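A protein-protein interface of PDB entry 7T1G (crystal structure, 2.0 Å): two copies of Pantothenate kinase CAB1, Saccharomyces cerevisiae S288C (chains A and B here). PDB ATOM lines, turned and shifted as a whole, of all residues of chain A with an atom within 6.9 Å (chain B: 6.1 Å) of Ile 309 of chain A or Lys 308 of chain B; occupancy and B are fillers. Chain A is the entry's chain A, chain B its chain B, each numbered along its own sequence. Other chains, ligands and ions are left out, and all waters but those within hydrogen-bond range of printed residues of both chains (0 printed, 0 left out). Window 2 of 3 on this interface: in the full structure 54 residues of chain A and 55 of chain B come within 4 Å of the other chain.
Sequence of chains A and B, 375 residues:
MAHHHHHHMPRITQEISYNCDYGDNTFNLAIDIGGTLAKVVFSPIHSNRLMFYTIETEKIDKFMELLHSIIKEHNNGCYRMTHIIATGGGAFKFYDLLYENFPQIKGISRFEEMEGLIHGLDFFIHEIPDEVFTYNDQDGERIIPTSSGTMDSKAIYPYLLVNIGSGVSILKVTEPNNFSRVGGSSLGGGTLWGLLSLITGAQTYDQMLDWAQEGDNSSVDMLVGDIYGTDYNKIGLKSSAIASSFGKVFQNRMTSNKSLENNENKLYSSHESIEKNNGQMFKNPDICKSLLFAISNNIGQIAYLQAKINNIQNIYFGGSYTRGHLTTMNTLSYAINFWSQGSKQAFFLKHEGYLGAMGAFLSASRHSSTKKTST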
ATOM      1  N   ILE A 302      -3.486 -23.420 -30.188  1.00  0.00           N
ATOM      2  CA  ILE A 302      -2.123 -23.264 -29.705  1.00  0.00           C
ATOM      3  C   ILE A 302      -1.228 -23.046 -30.926  1.00  0.00           C
ATOM      4  O   ILE A 302      -0.365 -22.170 -30.924  1.00  0.00           O
ATOM      5  CB  ILE A 302      -1.671 -24.475 -28.849  1.00  0.00           C
ATOM      6  CG1 ILE A 302      -2.532 -24.677 -27.594  1.00  0.00           C
ATOM      7  CG2 ILE A 302      -0.197 -24.378 -28.484  1.00  0.00           C
ATOM      8  CD1 ILE A 302      -2.245 -23.685 -26.508  1.00  0.00           C
ATOM      9  N   TYR A 304      -2.149 -21.845 -33.804  1.00  0.00           N
ATOM     10  CA  TYR A 304      -2.476 -20.511 -34.286  1.00  0.00           C
ATOM     11  C   TYR A 304      -1.679 -19.462 -33.522  1.00  0.00           C
ATOM     12  O   TYR A 304      -1.032 -18.603 -34.123  1.00  0.00           O
ATOM     13  CB  TYR A 304      -3.987 -20.216 -34.249  1.00  0.00           C
ATOM     14  CG  TYR A 304      -4.245 -18.729 -34.285  1.00  0.00           C
ATOM     15  CD1 TYR A 304      -4.005 -17.991 -35.444  1.00  0.00           C
ATOM     16  CD2 TYR A 304      -4.640 -18.056 -33.139  1.00  0.00           C
ATOM     17  CE1 TYR A 304      -4.179 -16.613 -35.465  1.00  0.00           C
ATOM     18  CE2 TYR A 304      -4.820 -16.675 -33.140  1.00  0.00           C
ATOM     19  CZ  TYR A 304      -4.586 -15.959 -34.305  1.00  0.00           C
ATOM     20  OH  TYR A 304      -4.749 -14.601 -34.260  1.00  0.00           O
ATOM     21  N   LEU A 305      -1.746 -19.540 -32.187  1.00  0.00           N
ATOM     22  CA  LEU A 305      -1.134 -18.535 -31.334  1.00  0.00           C
ATOM     23  C   LEU A 305       0.378 -18.500 -31.564  1.00  0.00           C
ATOM     24  O   LEU A 305       0.978 -17.418 -31.651  1.00  0.00           O
ATOM     25  CB  LEU A 305      -1.516 -18.808 -29.868  1.00  0.00           C
ATOM     26  CG  LEU A 305      -2.992 -18.637 -29.497  1.00  0.00           C
ATOM     27  CD1 LEU A 305      -3.284 -19.205 -28.102  1.00  0.00           C
ATOM     28  CD2 LEU A 305      -3.405 -17.160 -29.547  1.00  0.00           C
ATOM     29  N   GLN A 306       0.982 -19.689 -31.748  1.00  0.00           N
ATOM     30  CA  GLN A 306       2.409 -19.788 -31.966  1.00  0.00           C
ATOM     31  C   GLN A 306       2.747 -19.186 -33.339  1.00  0.00           C
ATOM     32  O   GLN A 306       3.764 -18.516 -33.484  1.00  0.00           O
ATOM     33  CB  GLN A 306       2.897 -21.230 -31.767  1.00  0.00           C
ATOM     34  CG  GLN A 306       2.916 -21.664 -30.283  1.00  0.00           C
ATOM     35  CD  GLN A 306       3.954 -21.006 -29.389  1.00  0.00           C
ATOM     36  OE1 GLN A 306       4.279 -19.836 -29.544  1.00  0.00           O
ATOM     37  NE2 GLN A 306       4.435 -21.722 -28.380  1.00  0.00           N
ATOM     38  N   ALA A 307       1.902 -19.453 -34.337  1.00  0.00           N
ATOM     39  CA  ALA A 307       2.110 -18.927 -35.682  1.00  0.00           C
ATOM     40  C   ALA A 307       1.946 -17.399 -35.678  1.00  0.00           C
ATOM     41  O   ALA A 307       2.752 -16.707 -36.297  1.00  0.00           O
ATOM     42  CB  ALA A 307       1.182 -19.599 -36.685  1.00  0.00           C
ATOM     43  N   LYS A 308       0.994 -16.907 -34.875  1.00  0.00           N
ATOM     44  CA  LYS A 308       0.734 -15.480 -34.704  1.00  0.00           C
ATOM     45  C   LYS A 308       1.967 -14.760 -34.144  1.00  0.00           C
ATOM     46  O   LYS A 308       2.420 -13.803 -34.761  1.00  0.00           O
ATOM     47  CB  LYS A 308      -0.540 -15.245 -33.876  1.00  0.00           C
ATOM     48  CG  LYS A 308      -0.828 -13.776 -33.574  1.00  0.00           C
ATOM     49  CD  LYS A 308      -1.402 -13.068 -34.766  1.00  0.00           C
ATOM     50  CE  LYS A 308      -1.649 -11.586 -34.518  1.00  0.00           C
ATOM     51  NZ  LYS A 308      -2.687 -11.099 -35.460  1.00  0.00           N
ATOM     52  N   ILE A 309       2.559 -15.268 -33.042  1.00  0.00           N
ATOM     53  CA  ILE A 309       3.748 -14.721 -32.383  1.00  0.00           C
ATOM     54  C   ILE A 309       4.946 -14.690 -33.338  1.00  0.00           C
ATOM     55  O   ILE A 309       5.726 -13.743 -33.302  1.00  0.00           O
ATOM     56  CB  ILE A 309       4.044 -15.518 -31.089  1.00  0.00           C
ATOM     57  CG1 ILE A 309       3.000 -15.212 -30.013  1.00  0.00           C
ATOM     58  CG2 ILE A 309       5.453 -15.314 -30.512  1.00  0.00           C
ATOM     59  CD1 ILE A 309       2.746 -16.371 -29.085  1.00  0.00           C
ATOM     60  N   ASN A 310       5.056 -15.709 -34.209  1.00  0.00           N
ATOM     61  CA  ASN A 310       6.208 -15.967 -35.059  1.00  0.00           C
ATOM     62  C   ASN A 310       5.928 -15.472 -36.487  1.00  0.00           C
ATOM     63  O   ASN A 310       6.798 -15.526 -37.357  1.00  0.00           O
ATOM     64  CB  ASN A 310       6.598 -17.449 -34.939  1.00  0.00           C
ATOM     65  CG  ASN A 310       7.239 -17.722 -33.586  1.00  0.00           C
ATOM     66  OD1 ASN A 310       8.300 -17.170 -33.293  1.00  0.00           O
ATOM     67  ND2 ASN A 310       6.551 -18.437 -32.698  1.00  0.00           N
ATOM     68  N   ASN A 311       4.734 -14.905 -36.701  1.00  0.00           N
ATOM     69  CA  ASN A 311       4.372 -14.369 -38.009  1.00  0.00           C
ATOM     70  C   ASN A 311       4.621 -15.437 -39.079  1.00  0.00           C
ATOM     71  O   ASN A 311       5.428 -15.261 -39.991  1.00  0.00           O
ATOM     72  CB  ASN A 311       5.165 -13.113 -38.374  1.00  0.00           C
ATOM     73  CG  ASN A 311       4.571 -12.438 -39.596  1.00  0.00           C
ATOM     74  OD1 ASN A 311       3.353 -12.432 -39.770  1.00  0.00           O
ATOM     75  ND2 ASN A 311       5.424 -11.932 -40.468  1.00  0.00           N
ATOM     76  N   ILE A 312       3.950 -16.575 -38.907  1.00  0.00           N
ATOM     77  CA  ILE A 312       4.078 -17.677 -39.829  1.00  0.00           C
ATOM     78  C   ILE A 312       2.697 -17.953 -40.410  1.00  0.00           C
ATOM     79  O   ILE A 312       1.719 -18.105 -39.676  1.00  0.00           O
ATOM     80  CB  ILE A 312       4.663 -18.893 -39.076  1.00  0.00           C
ATOM     81  CG1 ILE A 312       6.149 -18.694 -38.768  1.00  0.00           C
ATOM     82  CG2 ILE A 312       4.397 -20.172 -39.880  1.00  0.00           C
ATOM     83  CD1 ILE A 312       6.713 -19.614 -37.674  1.00  0.00           C
ATOM     84  N   LYS A 344      -4.160 -17.872 -42.057  1.00  0.00           N
ATOM     85  CA  LYS A 344      -3.214 -18.979 -41.916  1.00  0.00           C
ATOM     86  C   LYS A 344      -3.835 -20.251 -42.481  1.00  0.00           C
ATOM     87  O   LYS A 344      -5.044 -20.279 -42.635  1.00  0.00           O
ATOM     88  CB  LYS A 344      -2.732 -19.128 -40.467  1.00  0.00           C
ATOM     89  CG  LYS A 344      -2.134 -17.843 -39.897  1.00  0.00           C
ATOM     90  CD  LYS A 344      -1.585 -17.940 -38.478  1.00  0.00           C
ATOM     91  CE  LYS A 344      -1.085 -16.614 -37.930  1.00  0.00           C
ATOM     92  NZ  LYS A 344      -0.003 -16.060 -38.787  1.00  0.00           N
ATOM     93  N   ALA B 303      -3.323 -18.248 -21.871  1.00  0.00           N
ATOM     94  CA  ALA B 303      -3.308 -16.926 -21.252  1.00  0.00           C
ATOM     95  C   ALA B 303      -1.967 -16.240 -21.518  1.00  0.00           C
ATOM     96  O   ALA B 303      -1.922 -15.039 -21.818  1.00  0.00           O
ATOM     97  CB  ALA B 303      -3.585 -17.042 -19.745  1.00  0.00           C
ATOM     98  N   TYR B 304      -0.873 -17.008 -21.367  1.00  0.00           N
ATOM     99  CA  TYR B 304       0.465 -16.464 -21.563  1.00  0.00           C
ATOM    100  C   TYR B 304       0.643 -16.089 -23.046  1.00  0.00           C
ATOM    101  O   TYR B 304       1.102 -15.007 -23.361  1.00  0.00           O
ATOM    102  CB  TYR B 304       1.549 -17.477 -21.140  1.00  0.00           C
ATOM    103  CG  TYR B 304       2.867 -17.144 -21.778  1.00  0.00           C
ATOM    104  CD1 TYR B 304       3.659 -16.132 -21.252  1.00  0.00           C
ATOM    105  CD2 TYR B 304       3.273 -17.764 -22.952  1.00  0.00           C
ATOM    106  CE1 TYR B 304       4.853 -15.770 -21.861  1.00  0.00           C
ATOM    107  CE2 TYR B 304       4.469 -17.415 -23.571  1.00  0.00           C
ATOM    108  CZ  TYR B 304       5.254 -16.411 -23.020  1.00  0.00           C
ATOM    109  OH  TYR B 304       6.434 -16.029 -23.576  1.00  0.00           O
ATOM    110  N   LEU B 305       0.226 -16.961 -23.962  1.00  0.00           N
ATOM    111  CA  LEU B 305       0.414 -16.670 -25.384  1.00  0.00           C
ATOM    112  C   LEU B 305      -0.394 -15.435 -25.822  1.00  0.00           C
ATOM    113  O   LEU B 305       0.107 -14.606 -26.568  1.00  0.00           O
ATOM    114  CB  LEU B 305       0.048 -17.927 -26.195  1.00  0.00           C
ATOM    115  CG  LEU B 305       1.003 -19.118 -25.991  1.00  0.00           C
ATOM    116  CD1 LEU B 305       0.399 -20.376 -26.616  1.00  0.00           C
ATOM    117  CD2 LEU B 305       2.378 -18.823 -26.587  1.00  0.00           C
ATOM    118  N   GLN B 306      -1.657 -15.340 -25.401  1.00  0.00           N
ATOM    119  CA  GLN B 306      -2.492 -14.166 -25.616  1.00  0.00           C
ATOM    120  C   GLN B 306      -1.819 -12.911 -25.041  1.00  0.00           C
ATOM    121  O   GLN B 306      -1.783 -11.877 -25.703  1.00  0.00           O
ATOM    122  CB  GLN B 306      -3.884 -14.380 -25.003  1.00  0.00           C
ATOM    123  CG  GLN B 306      -4.726 -15.465 -25.675  1.00  0.00           C
ATOM    124  CD  GLN B 306      -5.378 -15.078 -26.992  1.00  0.00           C
ATOM    125  OE1 GLN B 306      -5.061 -14.066 -27.595  1.00  0.00           O
ATOM    126  NE2 GLN B 306      -6.298 -15.903 -27.461  1.00  0.00           N
ATOM    127  N   ALA B 307      -1.291 -12.995 -23.811  1.00  0.00           N
ATOM    128  CA  ALA B 307      -0.606 -11.873 -23.172  1.00  0.00           C
ATOM    129  C   ALA B 307       0.602 -11.427 -23.997  1.00  0.00           C
ATOM    130  O   ALA B 307       0.840 -10.231 -24.129  1.00  0.00           O
ATOM    131  CB  ALA B 307      -0.164 -12.201 -21.762  1.00  0.00           C
ATOM    132  N   LYS B 308       1.351 -12.406 -24.511  1.00  0.00           N
ATOM    133  CA  LYS B 308       2.490 -12.147 -25.359  1.00  0.00           C
ATOM    134  C   LYS B 308       2.048 -11.419 -26.632  1.00  0.00           C
ATOM    135  O   LYS B 308       2.619 -10.389 -26.959  1.00  0.00           O
ATOM    136  CB  LYS B 308       3.195 -13.479 -25.650  1.00  0.00           C
ATOM    137  CG  LYS B 308       4.504 -13.378 -26.430  1.00  0.00           C
ATOM    138  CD  LYS B 308       5.706 -13.600 -25.530  1.00  0.00           C
ATOM    139  CE  LYS B 308       6.883 -14.243 -26.239  1.00  0.00           C
ATOM    140  NZ  LYS B 308       6.561 -15.606 -26.755  1.00  0.00           N
ATOM    141  N   ILE B 309       1.032 -11.931 -27.328  1.00  0.00           N
ATOM    142  CA  ILE B 309       0.538 -11.315 -28.563  1.00  0.00           C
ATOM    143  C   ILE B 309       0.128  -9.867 -28.287  1.00  0.00           C
ATOM    144  O   ILE B 309       0.353  -8.994 -29.112  1.00  0.00           O
ATOM    145  CB  ILE B 309      -0.636 -12.111 -29.168  1.00  0.00           C
ATOM    146  CG1 ILE B 309      -0.130 -13.438 -29.759  1.00  0.00           C
ATOM    147  CG2 ILE B 309      -1.408 -11.254 -30.197  1.00  0.00           C
ATOM    148  CD1 ILE B 309      -1.223 -14.434 -30.159  1.00  0.00           C
ATOM    149  N   ASN B 310      -0.453  -9.627 -27.102  1.00  0.00           N
ATOM    150  CA  ASN B 310      -1.108  -8.366 -26.808  1.00  0.00           C
ATOM    151  C   ASN B 310      -0.200  -7.465 -25.976  1.00  0.00           C
ATOM    152  O   ASN B 310      -0.641  -6.422 -25.559  1.00  0.00           O
ATOM    153  CB  ASN B 310      -2.476  -8.595 -26.153  1.00  0.00           C
ATOM    154  CG  ASN B 310      -3.478  -9.086 -27.174  1.00  0.00           C
ATOM    155  OD1 ASN B 310      -3.858  -8.331 -28.052  1.00  0.00           O
ATOM    156  ND2 ASN B 310      -3.878 -10.343 -27.111  1.00  0.00           N
ATOM    157  N   ASN B 311       1.031  -7.905 -25.685  1.00  0.00           N
ATOM    158  CA  ASN B 311       2.035  -7.121 -24.977  1.00  0.00           C
ATOM    159  C   ASN B 311       1.530  -6.736 -23.580  1.00  0.00           C
ATOM    160  O   ASN B 311       1.653  -5.586 -23.157  1.00  0.00           O
ATOM    161  CB  ASN B 311       2.523  -5.942 -25.834  1.00  0.00           C
ATOM    162  CG  ASN B 311       3.721  -5.247 -25.219  1.00  0.00           C
ATOM    163  OD1 ASN B 311       4.402  -5.836 -24.383  1.00  0.00           O
ATOM    164  ND2 ASN B 311       3.980  -4.000 -25.607  1.00  0.00           N
ATOM    165  N   ILE B 312       0.927  -7.706 -22.875  1.00  0.00           N
ATOM    166  CA  ILE B 312       0.380  -7.486 -21.549  1.00  0.00           C
ATOM    167  C   ILE B 312       1.211  -8.269 -20.524  1.00  0.00           C
ATOM    168  O   ILE B 312       1.615  -9.387 -20.792  1.00  0.00           O
ATOM    169  CB  ILE B 312      -1.115  -7.859 -21.546  1.00  0.00           C
ATOM    170  CG1 ILE B 312      -1.898  -6.868 -22.403  1.00  0.00           C
ATOM    171  CG2 ILE B 312      -1.666  -7.930 -20.117  1.00  0.00           C
ATOM    172  CD1 ILE B 312      -3.287  -7.324 -22.795  1.00  0.00           C
ATOM    173  N   LYS B 344       5.840 -12.036 -16.514  1.00  0.00           N
ATOM    174  CA  LYS B 344       4.403 -11.780 -16.447  1.00  0.00           C
ATOM    175  C   LYS B 344       3.920 -12.264 -15.085  1.00  0.00           C
ATOM    176  O   LYS B 344       4.607 -13.074 -14.464  1.00  0.00           O
ATOM    177  CB  LYS B 344       3.642 -12.369 -17.654  1.00  0.00           C
ATOM    178  CG  LYS B 344       4.047 -11.810 -19.016  1.00  0.00           C
ATOM    179  CD  LYS B 344       3.192 -12.307 -20.180  1.00  0.00           C
ATOM    180  CE  LYS B 344       3.862 -12.130 -21.535  1.00  0.00           C
ATOM    181  NZ  LYS B 344       3.910 -10.683 -21.860  1.00  0.00           N
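O of Gln 306 of chain A lies within hydrogen-bond range of ND2 of Asn 310 of chain A, 2.9 Å away.
O of Gln 306 of chain B lies within hydrogen-bond range of ND2 of Asn 310 of chain B (3.0 Å).
The side-chain hydroxyl of Tyr 304 of chain B lies close to the side-chain amino group of Lys 308 of chain B, 3.2 Å away.
Leu 305 of chain A touches Gln 306 of chain B (CD2 to NE2, 3.8 Å).
Ile 309 of chain B touches Leu 305 of chain A (CD1 to CD2, 3.5 Å).
OE1 of Gln 306 of chain A touches CD2 of Leu 305 of chain B (3.7 Å).
CG of Lys 308 of chain A touches CD1 of Ile 309 of chain B, 3.5 Å away.
CD1 of Ile 309 of chain A touches CD2 of Leu 305 of chain B, 3.5 Å away.
Lys 308 of chain B touches Ile 309 of chain A (NZ to CG2, 3.9 Å).
CG1 of Ile 309 of chain B touches CG1 of Ile 309 of chain A, at 3.6 Å.
Printed residues of chain B within 4 Å of Leu 305 of chain A: Gln 306 (3.8 Å) and Ile 309 (3.5 Å).
Printed residues of chain B within 4 Å of Lys 308 of chain A: Ile 309 (3.5 Å).
Of chain B, only Leu 305 (3.5 Å), Lys 308 (3.9 Å) and Ile 309 (3.6 Å) come within 4 Å of Ile 309 of chain A.
Printed residues of chain A within 4 Å of Leu 305 of chain B: Gln 306 (3.7 Å) and Ile 309 (3.5 Å).
Of the printed residues of chain A, Gln 306 of chain B touches Leu 305.
Hydrophobic or aromatic side chains of chain A within 4 Å of the printed part of chain B: Leu 305 and Ile 309.
Hydrophobic or aromatic side chains of chain B that line the printed part of chain A: Leu 305 and Ile 309.
Leu 305 of chain A touches Gln 306 of chain B, and with the chains exchanged Gln 306 of chain A touches Leu 305 of chain B.
Leu 305 of chain A touches Ile 309 of chain B, and with the chains exchanged Ile 309 of chain A touches Leu 305 of chain B.
Lys 308 of chain A touches Ile 309 of chain B, and with the chains exchanged Ile 309 of chain A touches Lys 308 of chain B.
Ile 309 of chain B touches its own counterpart, Ile 309 of chain A.
10 positions are printed for both chains.
Of the 7 pairs that touch across the chains among the printed residues, 7 have their exchanged pair printed and touching as well.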
